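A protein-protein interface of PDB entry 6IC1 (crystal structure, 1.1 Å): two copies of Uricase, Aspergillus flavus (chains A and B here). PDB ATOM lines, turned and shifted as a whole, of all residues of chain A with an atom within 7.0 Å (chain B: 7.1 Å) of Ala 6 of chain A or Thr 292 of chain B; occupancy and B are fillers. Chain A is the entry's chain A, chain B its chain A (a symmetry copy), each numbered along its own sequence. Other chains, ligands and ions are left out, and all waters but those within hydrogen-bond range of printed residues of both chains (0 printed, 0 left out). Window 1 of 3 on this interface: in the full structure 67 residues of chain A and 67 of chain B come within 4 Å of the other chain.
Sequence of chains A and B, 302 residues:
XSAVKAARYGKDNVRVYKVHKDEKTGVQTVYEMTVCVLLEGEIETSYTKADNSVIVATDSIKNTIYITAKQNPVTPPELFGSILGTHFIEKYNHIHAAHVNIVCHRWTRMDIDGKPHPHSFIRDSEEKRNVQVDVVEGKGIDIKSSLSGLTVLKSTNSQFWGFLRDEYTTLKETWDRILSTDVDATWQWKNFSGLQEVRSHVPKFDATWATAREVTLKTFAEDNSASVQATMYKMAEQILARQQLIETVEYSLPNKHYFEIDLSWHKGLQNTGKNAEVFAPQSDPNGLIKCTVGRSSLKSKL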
ATOM      1  N   ALA A   3       0.922  12.052 -22.947  1.00  0.00           N
ATOM      2  CA  ALA A   3      -0.332  12.302 -22.297  1.00  0.00           C
ATOM      3  C   ALA A   3      -1.374  11.238 -22.591  1.00  0.00           C
ATOM      4  O   ALA A   3      -1.372  10.557 -23.636  1.00  0.00           O
ATOM      5  CB  ALA A   3      -0.894  13.694 -22.565  1.00  0.00           C
ATOM      6  N   VAL A   4      -2.240  11.051 -21.624  1.00  0.00           N
ATOM      7  CA  VAL A   4      -3.353  10.136 -21.775  1.00  0.00           C
ATOM      8  C   VAL A   4      -4.369  10.715 -22.758  1.00  0.00           C
ATOM      9  O   VAL A   4      -4.945  11.790 -22.518  1.00  0.00           O
ATOM     10  CB  VAL A   4      -3.999   9.827 -20.438  1.00  0.00           C
ATOM     11  CG1 VAL A   4      -5.218   8.925 -20.624  1.00  0.00           C
ATOM     12  CG2 VAL A   4      -3.019   9.179 -19.467  1.00  0.00           C
ATOM     13  N   LYS A   5      -4.583  10.040 -23.863  1.00  0.00           N
ATOM     14  CA  LYS A   5      -5.585  10.425 -24.864  1.00  0.00           C
ATOM     15  C   LYS A   5      -6.931   9.779 -24.612  1.00  0.00           C
ATOM     16  O   LYS A   5      -8.020  10.360 -24.929  1.00  0.00           O
ATOM     17  CB  LYS A   5      -5.093  10.083 -26.264  1.00  0.00           C
ATOM     18  CG  LYS A   5      -3.802  10.790 -26.614  1.00  0.00           C
ATOM     19  CD  LYS A   5      -3.826  12.356 -26.540  1.00  0.00           C
ATOM     20  CE  LYS A   5      -2.421  12.911 -26.867  1.00  0.00           C
ATOM     21  NZ  LYS A   5      -2.385  14.404 -26.843  1.00  0.00           N
ATOM     22  N   ALA A   6      -6.944   8.574 -24.064  1.00  0.00           N
ATOM     23  CA  ALA A   6      -8.183   7.858 -23.728  1.00  0.00           C
ATOM     24  C   ALA A   6      -7.827   6.932 -22.575  1.00  0.00           C
ATOM     25  O   ALA A   6      -6.726   6.415 -22.505  1.00  0.00           O
ATOM     26  CB  ALA A   6      -8.697   7.040 -24.901  1.00  0.00           C
ATOM     27  N   ALA A   7      -8.819   6.671 -21.734  1.00  0.00           N
ATOM     28  CA  ALA A   7      -8.607   5.714 -20.621  1.00  0.00           C
ATOM     29  C   ALA A   7      -9.986   5.240 -20.170  1.00  0.00           C
ATOM     30  O   ALA A   7     -10.927   6.019 -20.050  1.00  0.00           O
ATOM     31  CB  ALA A   7      -7.876   6.309 -19.473  1.00  0.00           C
ATOM     32  N   ARG A   8     -10.068   3.954 -19.892  1.00  0.00           N
ATOM     33  CA  ARG A   8     -11.236   3.384 -19.215  1.00  0.00           C
ATOM     34  C   ARG A   8     -10.798   2.165 -18.435  1.00  0.00           C
ATOM     35  O   ARG A   8      -9.789   1.518 -18.833  1.00  0.00           O
ATOM     36  CB  ARG A   8     -12.396   3.087 -20.129  1.00  0.00           C
ATOM     37  CG  ARG A   8     -12.158   2.023 -21.139  1.00  0.00           C
ATOM     38  CD  ARG A   8     -13.382   1.794 -22.021  1.00  0.00           C
ATOM     39  NE  ARG A   8     -13.716   2.945 -22.810  1.00  0.00           N
ATOM     40  CZ  ARG A   8     -14.733   3.063 -23.667  1.00  0.00           C
ATOM     41  NH1 ARG A   8     -15.629   2.103 -23.800  1.00  0.00           N
ATOM     42  NH2 ARG A   8     -14.907   4.163 -24.393  1.00  0.00           N
ATOM     43  N   GLU A  40     -14.948   5.864 -17.214  1.00  0.00           N
ATOM     44  CA  GLU A  40     -14.118   6.949 -17.686  1.00  0.00           C
ATOM     45  C   GLU A  40     -14.372   8.177 -16.833  1.00  0.00           C
ATOM     46  O   GLU A  40     -15.466   8.346 -16.281  1.00  0.00           O
ATOM     47  CB  GLU A  40     -14.456   7.390 -19.123  1.00  0.00           C
ATOM     48  CG  GLU A  40     -14.288   6.410 -20.199  1.00  0.00           C
ATOM     49  CD  GLU A  40     -14.584   7.099 -21.535  1.00  0.00           C
ATOM     50  OE1 GLU A  40     -13.824   7.978 -21.981  1.00  0.00           O
ATOM     51  OE2 GLU A  40     -15.655   6.879 -22.060  1.00  0.00           O
ATOM     52  N   TYR A  47      -2.800   7.067 -13.988  1.00  0.00           N
ATOM     53  CA  TYR A  47      -1.838   6.588 -14.975  1.00  0.00           C
ATOM     54  C   TYR A  47      -0.551   7.387 -14.908  1.00  0.00           C
ATOM     55  O   TYR A  47       0.545   6.780 -14.988  1.00  0.00           O
ATOM     56  CB  TYR A  47      -2.436   6.680 -16.410  1.00  0.00           C
ATOM     57  CG  TYR A  47      -3.653   5.824 -16.609  1.00  0.00           C
ATOM     58  CD1 TYR A  47      -4.917   6.247 -16.263  1.00  0.00           C
ATOM     59  CD2 TYR A  47      -3.574   4.534 -17.153  1.00  0.00           C
ATOM     60  CE1 TYR A  47      -6.059   5.500 -16.471  1.00  0.00           C
ATOM     61  CE2 TYR A  47      -4.702   3.778 -17.373  1.00  0.00           C
ATOM     62  CZ  TYR A  47      -5.970   4.240 -17.063  1.00  0.00           C
ATOM     63  OH  TYR A  47      -7.120   3.541 -17.290  1.00  0.00           O
ATOM     64  N   THR B 186      -0.781  -2.108 -28.546  1.00  0.00           N
ATOM     65  CA  THR B 186      -0.978  -1.696 -29.944  1.00  0.00           C
ATOM     66  C   THR B 186      -0.241  -0.388 -30.161  1.00  0.00           C
ATOM     67  O   THR B 186      -0.436   0.555 -29.377  1.00  0.00           O
ATOM     68  CB  THR B 186      -2.445  -1.528 -30.243  1.00  0.00           C
ATOM     69  OG1 THR B 186      -3.129  -2.744 -29.983  1.00  0.00           O
ATOM     70  CG2 THR B 186      -2.742  -1.107 -31.659  1.00  0.00           C
ATOM     71  N   MET B 232       1.484   0.527 -16.840  1.00  0.00           N
ATOM     72  CA  MET B 232       1.247   0.478 -18.284  1.00  0.00           C
ATOM     73  C   MET B 232       1.559   1.833 -18.933  1.00  0.00           C
ATOM     74  O   MET B 232       2.033   1.872 -20.073  1.00  0.00           O
ATOM     75  CB  MET B 232      -0.183   0.018 -18.569  1.00  0.00           C
ATOM     76  CG  MET B 232      -1.259   1.025 -18.261  1.00  0.00           C
ATOM     77  SD  MET B 232      -2.897   0.369 -17.962  1.00  0.00           S
ATOM     78  CE  MET B 232      -3.321  -0.362 -19.528  1.00  0.00           C
ATOM     79  N   TYR B 233       1.337   2.922 -18.219  1.00  0.00           N
ATOM     80  CA  TYR B 233       1.610   4.228 -18.790  1.00  0.00           C
ATOM     81  C   TYR B 233       3.086   4.376 -19.045  1.00  0.00           C
ATOM     82  O   TYR B 233       3.515   4.935 -20.079  1.00  0.00           O
ATOM     83  CB  TYR B 233       1.084   5.318 -17.854  1.00  0.00           C
ATOM     84  CG  TYR B 233       1.275   6.711 -18.392  1.00  0.00           C
ATOM     85  CD1 TYR B 233       0.399   7.232 -19.318  1.00  0.00           C
ATOM     86  CD2 TYR B 233       2.400   7.442 -18.075  1.00  0.00           C
ATOM     87  CE1 TYR B 233       0.580   8.486 -19.888  1.00  0.00           C
ATOM     88  CE2 TYR B 233       2.620   8.696 -18.642  1.00  0.00           C
ATOM     89  CZ  TYR B 233       1.699   9.178 -19.562  1.00  0.00           C
ATOM     90  OH  TYR B 233       1.870  10.448 -20.114  1.00  0.00           O
ATOM     91  N   ALA B 236       4.016   2.682 -22.272  1.00  0.00           N
ATOM     92  CA  ALA B 236       3.552   3.438 -23.461  1.00  0.00           C
ATOM     93  C   ALA B 236       4.497   4.631 -23.675  1.00  0.00           C
ATOM     94  O   ALA B 236       4.860   4.923 -24.852  1.00  0.00           O
ATOM     95  CB  ALA B 236       2.129   3.843 -23.323  1.00  0.00           C
ATOM     96  N   LEU B 240       6.681   5.389 -27.210  1.00  0.00           N
ATOM     97  CA  LEU B 240       6.562   6.638 -28.003  1.00  0.00           C
ATOM     98  C   LEU B 240       7.905   7.326 -28.108  1.00  0.00           C
ATOM     99  O   LEU B 240       8.205   7.914 -29.171  1.00  0.00           O
ATOM    100  CB  LEU B 240       5.531   7.550 -27.362  1.00  0.00           C
ATOM    101  CG  LEU B 240       4.110   7.092 -27.517  1.00  0.00           C
ATOM    102  CD1 LEU B 240       3.187   7.867 -26.615  1.00  0.00           C
ATOM    103  CD2 LEU B 240       3.617   7.235 -28.968  1.00  0.00           C
ATOM    104  N   GLU B 247       2.152   7.301 -33.519  1.00  0.00           N
ATOM    105  CA  GLU B 247       1.359   8.405 -32.955  1.00  0.00           C
ATOM    106  C   GLU B 247       0.803   8.057 -31.561  1.00  0.00           C
ATOM    107  O   GLU B 247       0.753   8.945 -30.703  1.00  0.00           O
ATOM    108  CB  GLU B 247       0.229   8.785 -33.884  1.00  0.00           C
ATOM    109  CG  GLU B 247       0.762   9.409 -35.170  1.00  0.00           C
ATOM    110  CD  GLU B 247      -0.274   9.809 -36.167  1.00  0.00           C
ATOM    111  OE1 GLU B 247      -1.432   9.354 -36.102  1.00  0.00           O
ATOM    112  OE2 GLU B 247       0.152  10.572 -37.088  1.00  0.00           O
ATOM    113  N   THR B 248       0.319   6.839 -31.373  1.00  0.00           N
ATOM    114  CA  THR B 248      -0.242   6.451 -30.087  1.00  0.00           C
ATOM    115  C   THR B 248       0.172   5.030 -29.761  1.00  0.00           C
ATOM    116  O   THR B 248       0.498   4.231 -30.659  1.00  0.00           O
ATOM    117  CB  THR B 248      -1.756   6.558 -30.044  1.00  0.00           C
ATOM    118  OG1 THR B 248      -2.353   5.666 -30.978  1.00  0.00           O
ATOM    119  CG2 THR B 248      -2.280   7.954 -30.299  1.00  0.00           C
ATOM    120  N   VAL B 249       0.157   4.727 -28.467  1.00  0.00           N
ATOM    121  CA  VAL B 249       0.307   3.363 -27.952  1.00  0.00           C
ATOM    122  C   VAL B 249      -0.898   3.087 -27.063  1.00  0.00           C
ATOM    123  O   VAL B 249      -1.204   3.897 -26.169  1.00  0.00           O
ATOM    124  CB  VAL B 249       1.637   3.207 -27.199  1.00  0.00           C
ATOM    125  CG1 VAL B 249       1.759   1.862 -26.567  1.00  0.00           C
ATOM    126  CG2 VAL B 249       2.778   3.489 -28.108  1.00  0.00           C
ATOM    127  N   GLU B 250      -1.486   1.935 -27.237  1.00  0.00           N
ATOM    128  CA  GLU B 250      -2.680   1.511 -26.475  1.00  0.00           C
ATOM    129  C   GLU B 250      -2.301   0.239 -25.719  1.00  0.00           C
ATOM    130  O   GLU B 250      -1.717  -0.676 -26.322  1.00  0.00           O
ATOM    131  CB  GLU B 250      -3.902   1.086 -27.308  1.00  0.00           C
ATOM    132  CG  GLU B 250      -4.298   2.055 -28.401  1.00  0.00           C
ATOM    133  CD  GLU B 250      -5.342   1.533 -29.364  1.00  0.00           C
ATOM    134  OE1 GLU B 250      -5.440   2.153 -30.411  1.00  0.00           O
ATOM    135  OE2 GLU B 250      -5.920   0.432 -29.123  1.00  0.00           O
ATOM    136  N   TYR B 251      -2.653   0.136 -24.462  1.00  0.00           N
ATOM    137  CA  TYR B 251      -2.595  -1.135 -23.727  1.00  0.00           C
ATOM    138  C   TYR B 251      -3.973  -1.506 -23.239  1.00  0.00           C
ATOM    139  O   TYR B 251      -4.763  -0.615 -22.820  1.00  0.00           O
ATOM    140  CB  TYR B 251      -1.653  -1.036 -22.524  1.00  0.00           C
ATOM    141  CG  TYR B 251      -0.194  -1.201 -22.840  1.00  0.00           C
ATOM    142  CD1 TYR B 251       0.603  -0.183 -23.286  1.00  0.00           C
ATOM    143  CD2 TYR B 251       0.426  -2.440 -22.665  1.00  0.00           C
ATOM    144  CE1 TYR B 251       1.930  -0.392 -23.611  1.00  0.00           C
ATOM    145  CE2 TYR B 251       1.765  -2.642 -22.956  1.00  0.00           C
ATOM    146  CZ  TYR B 251       2.518  -1.613 -23.445  1.00  0.00           C
ATOM    147  OH  TYR B 251       3.834  -1.774 -23.768  1.00  0.00           O
ATOM    148  N   LYS B 290      -7.410  -0.052 -19.345  1.00  0.00           N
ATOM    149  CA  LYS B 290      -7.081   0.373 -20.712  1.00  0.00           C
ATOM    150  C   LYS B 290      -6.599   1.796 -20.708  1.00  0.00           C
ATOM    151  O   LYS B 290      -7.063   2.665 -19.950  1.00  0.00           O
ATOM    152  CB  LYS B 290      -8.316   0.289 -21.604  1.00  0.00           C
ATOM    153  CG  LYS B 290      -8.931  -1.091 -21.705  1.00  0.00           C
ATOM    154  CD  LYS B 290     -10.164  -1.146 -22.635  1.00  0.00           C
ATOM    155  CE  LYS B 290     -10.778  -2.487 -22.677  1.00  0.00           C
ATOM    156  NZ  LYS B 290     -11.359  -2.879 -23.883  1.00  0.00           N
ATOM    157  N   CYS B 291      -5.576   2.054 -21.555  1.00  0.00           N
ATOM    158  CA  CYS B 291      -5.010   3.421 -21.756  1.00  0.00           C
ATOM    159  C   CYS B 291      -4.727   3.553 -23.287  1.00  0.00           C
ATOM    160  O   CYS B 291      -4.312   2.560 -23.906  1.00  0.00           O
ATOM    161  CB  CYS B 291      -3.736   3.589 -20.867  1.00  0.00           C
ATOM    162  SG  CYS B 291      -3.356   5.322 -20.583  1.00  0.00           S
ATOM    163  N   THR B 292      -4.901   4.725 -23.878  1.00  0.00           N
ATOM    164  CA  THR B 292      -4.284   5.153 -25.134  1.00  0.00           C
ATOM    165  C   THR B 292      -3.437   6.372 -24.812  1.00  0.00           C
ATOM    166  O   THR B 292      -3.977   7.358 -24.282  1.00  0.00           O
ATOM    167  CB  THR B 292      -5.292   5.509 -26.231  1.00  0.00           C
ATOM    168  OG1 THR B 292      -6.106   4.348 -26.421  1.00  0.00           O
ATOM    169  CG2 THR B 292      -4.583   5.878 -27.501  1.00  0.00           C
ATOM    170  N   VAL B 293      -2.158   6.307 -25.097  1.00  0.00           N
ATOM    171  CA  VAL B 293      -1.190   7.362 -24.786  1.00  0.00           C
ATOM    172  C   VAL B 293      -0.685   7.935 -26.092  1.00  0.00           C
ATOM    173  O   VAL B 293      -0.385   7.208 -27.037  1.00  0.00           O
ATOM    174  CB  VAL B 293      -0.042   6.817 -23.965  1.00  0.00           C
ATOM    175  CG1 VAL B 293       0.955   7.896 -23.625  1.00  0.00           C
ATOM    176  CG2 VAL B 293      -0.568   6.174 -22.687  1.00  0.00           C
ATOM    177  N   GLY B 294      -0.636   9.279 -26.164  1.00  0.00           N
ATOM    178  CA  GLY B 294      -0.078   9.976 -27.313  1.00  0.00           C
ATOM    179  C   GLY B 294       0.872  11.057 -26.931  1.00  0.00           C
ATOM    180  O   GLY B 294       1.256  11.075 -25.701  1.00  0.00           O
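The backbone NH (N) of Gly 294 of chain B lies within hydrogen-bond range of the backbone carbonyl oxygen (O) of Ala 3 of chain A.
The backbone NH of Lys 5 of chain A is in hydrogen-bond range of the backbone carbonyl oxygen of Thr 292 of chain B (2.8 Å).
The backbone NH of Ala 3 of chain A sits at hydrogen-bond distance from the side-chain hydroxyl of Tyr 233 of chain B, at 3.4 Å.
The backbone NH (N) of Thr 292 of chain B is in hydrogen-bond range of the backbone carbonyl oxygen (O) of Ala 6 of chain A, 2.8 Å away.
The backbone NH (N) of Lys 290 of chain B is in hydrogen-bond range of the backbone carbonyl oxygen (O) of Arg 8 of chain A (2.9 Å).
The backbone carbonyl oxygen of Lys 290 of chain B sits at hydrogen-bond distance from the side-chain hydroxyl of Tyr 47 of chain A (2.8 Å).
N of Tyr 251 of chain B lies within hydrogen-bond range of O of Cys 291 of chain B.
The side-chain carboxylate (OE2) of Glu 40 of chain A is in salt-bridge range of the guanidinium group (NH2) of Arg 8 of chain A (3.7 Å).
The backbone NH (N) of Val 293 of chain B sits at hydrogen-bond distance from the backbone carbonyl oxygen (O) of Val 249 of chain B, at 2.8 Å.
Among the printed residues, pairs that only touch across the chains: Ala 3 of chain A with Val 293 of chain B (3.4 Å), Val 4 of chain A with Tyr 233 of chain B (3.7 Å), Val 4 of chain A with Thr 292 of chain B (3.7 Å), Lys 5 of chain A with Gly 294 of chain B (3.5 Å), Ala 6 of chain A with Cys 291 of chain B (3.5 Å), Ala 7 of chain A with Lys 290 of chain B (3.5 Å), Tyr 47 of chain A with Met 232 of chain B (3.9 Å), Tyr 47 of chain A with Tyr 233 of chain B (3.3 Å) and Tyr 47 of chain A with Cys 291 of chain B (3.5 Å).
Of the printed residues of chain B, Ala 3 of chain A touches Tyr 233, Val 293 and Gly 294.
Of the printed residues of chain A, Cys 291 of chain B touches Ala 6 and Tyr 47.
Of chain A, only Val 4, Lys 5 and Ala 6 come within 4 Å of Thr 292 of chain B.
The nearest printed residue of chain B that does not touch Ala 6 of chain A is Lys 290 of chain B (4.6 Å).
The nearest residue of chain A that does not touch Thr 292 of chain B is Ala 3 of chain A (4.2 Å).
Of the 15 printed residues of chain B, 7 touch a printed residue of chain A.
Hydrophobic or aromatic side chains of chain B within 4 Å of the printed part of chain A: Met 232, Tyr 233 and Val 293.
Among the printed residues, 15 pairs touch across the chains.
Among the printed residues, no Asp or Glu carboxylate lies within 4 Å of a Lys or Arg side-chain nitrogen of the other chain.
No position is printed for both chains.
Of the 15 pairs that touch across the chains among the printed residues, none has its exchanged pair printed and touching as well.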
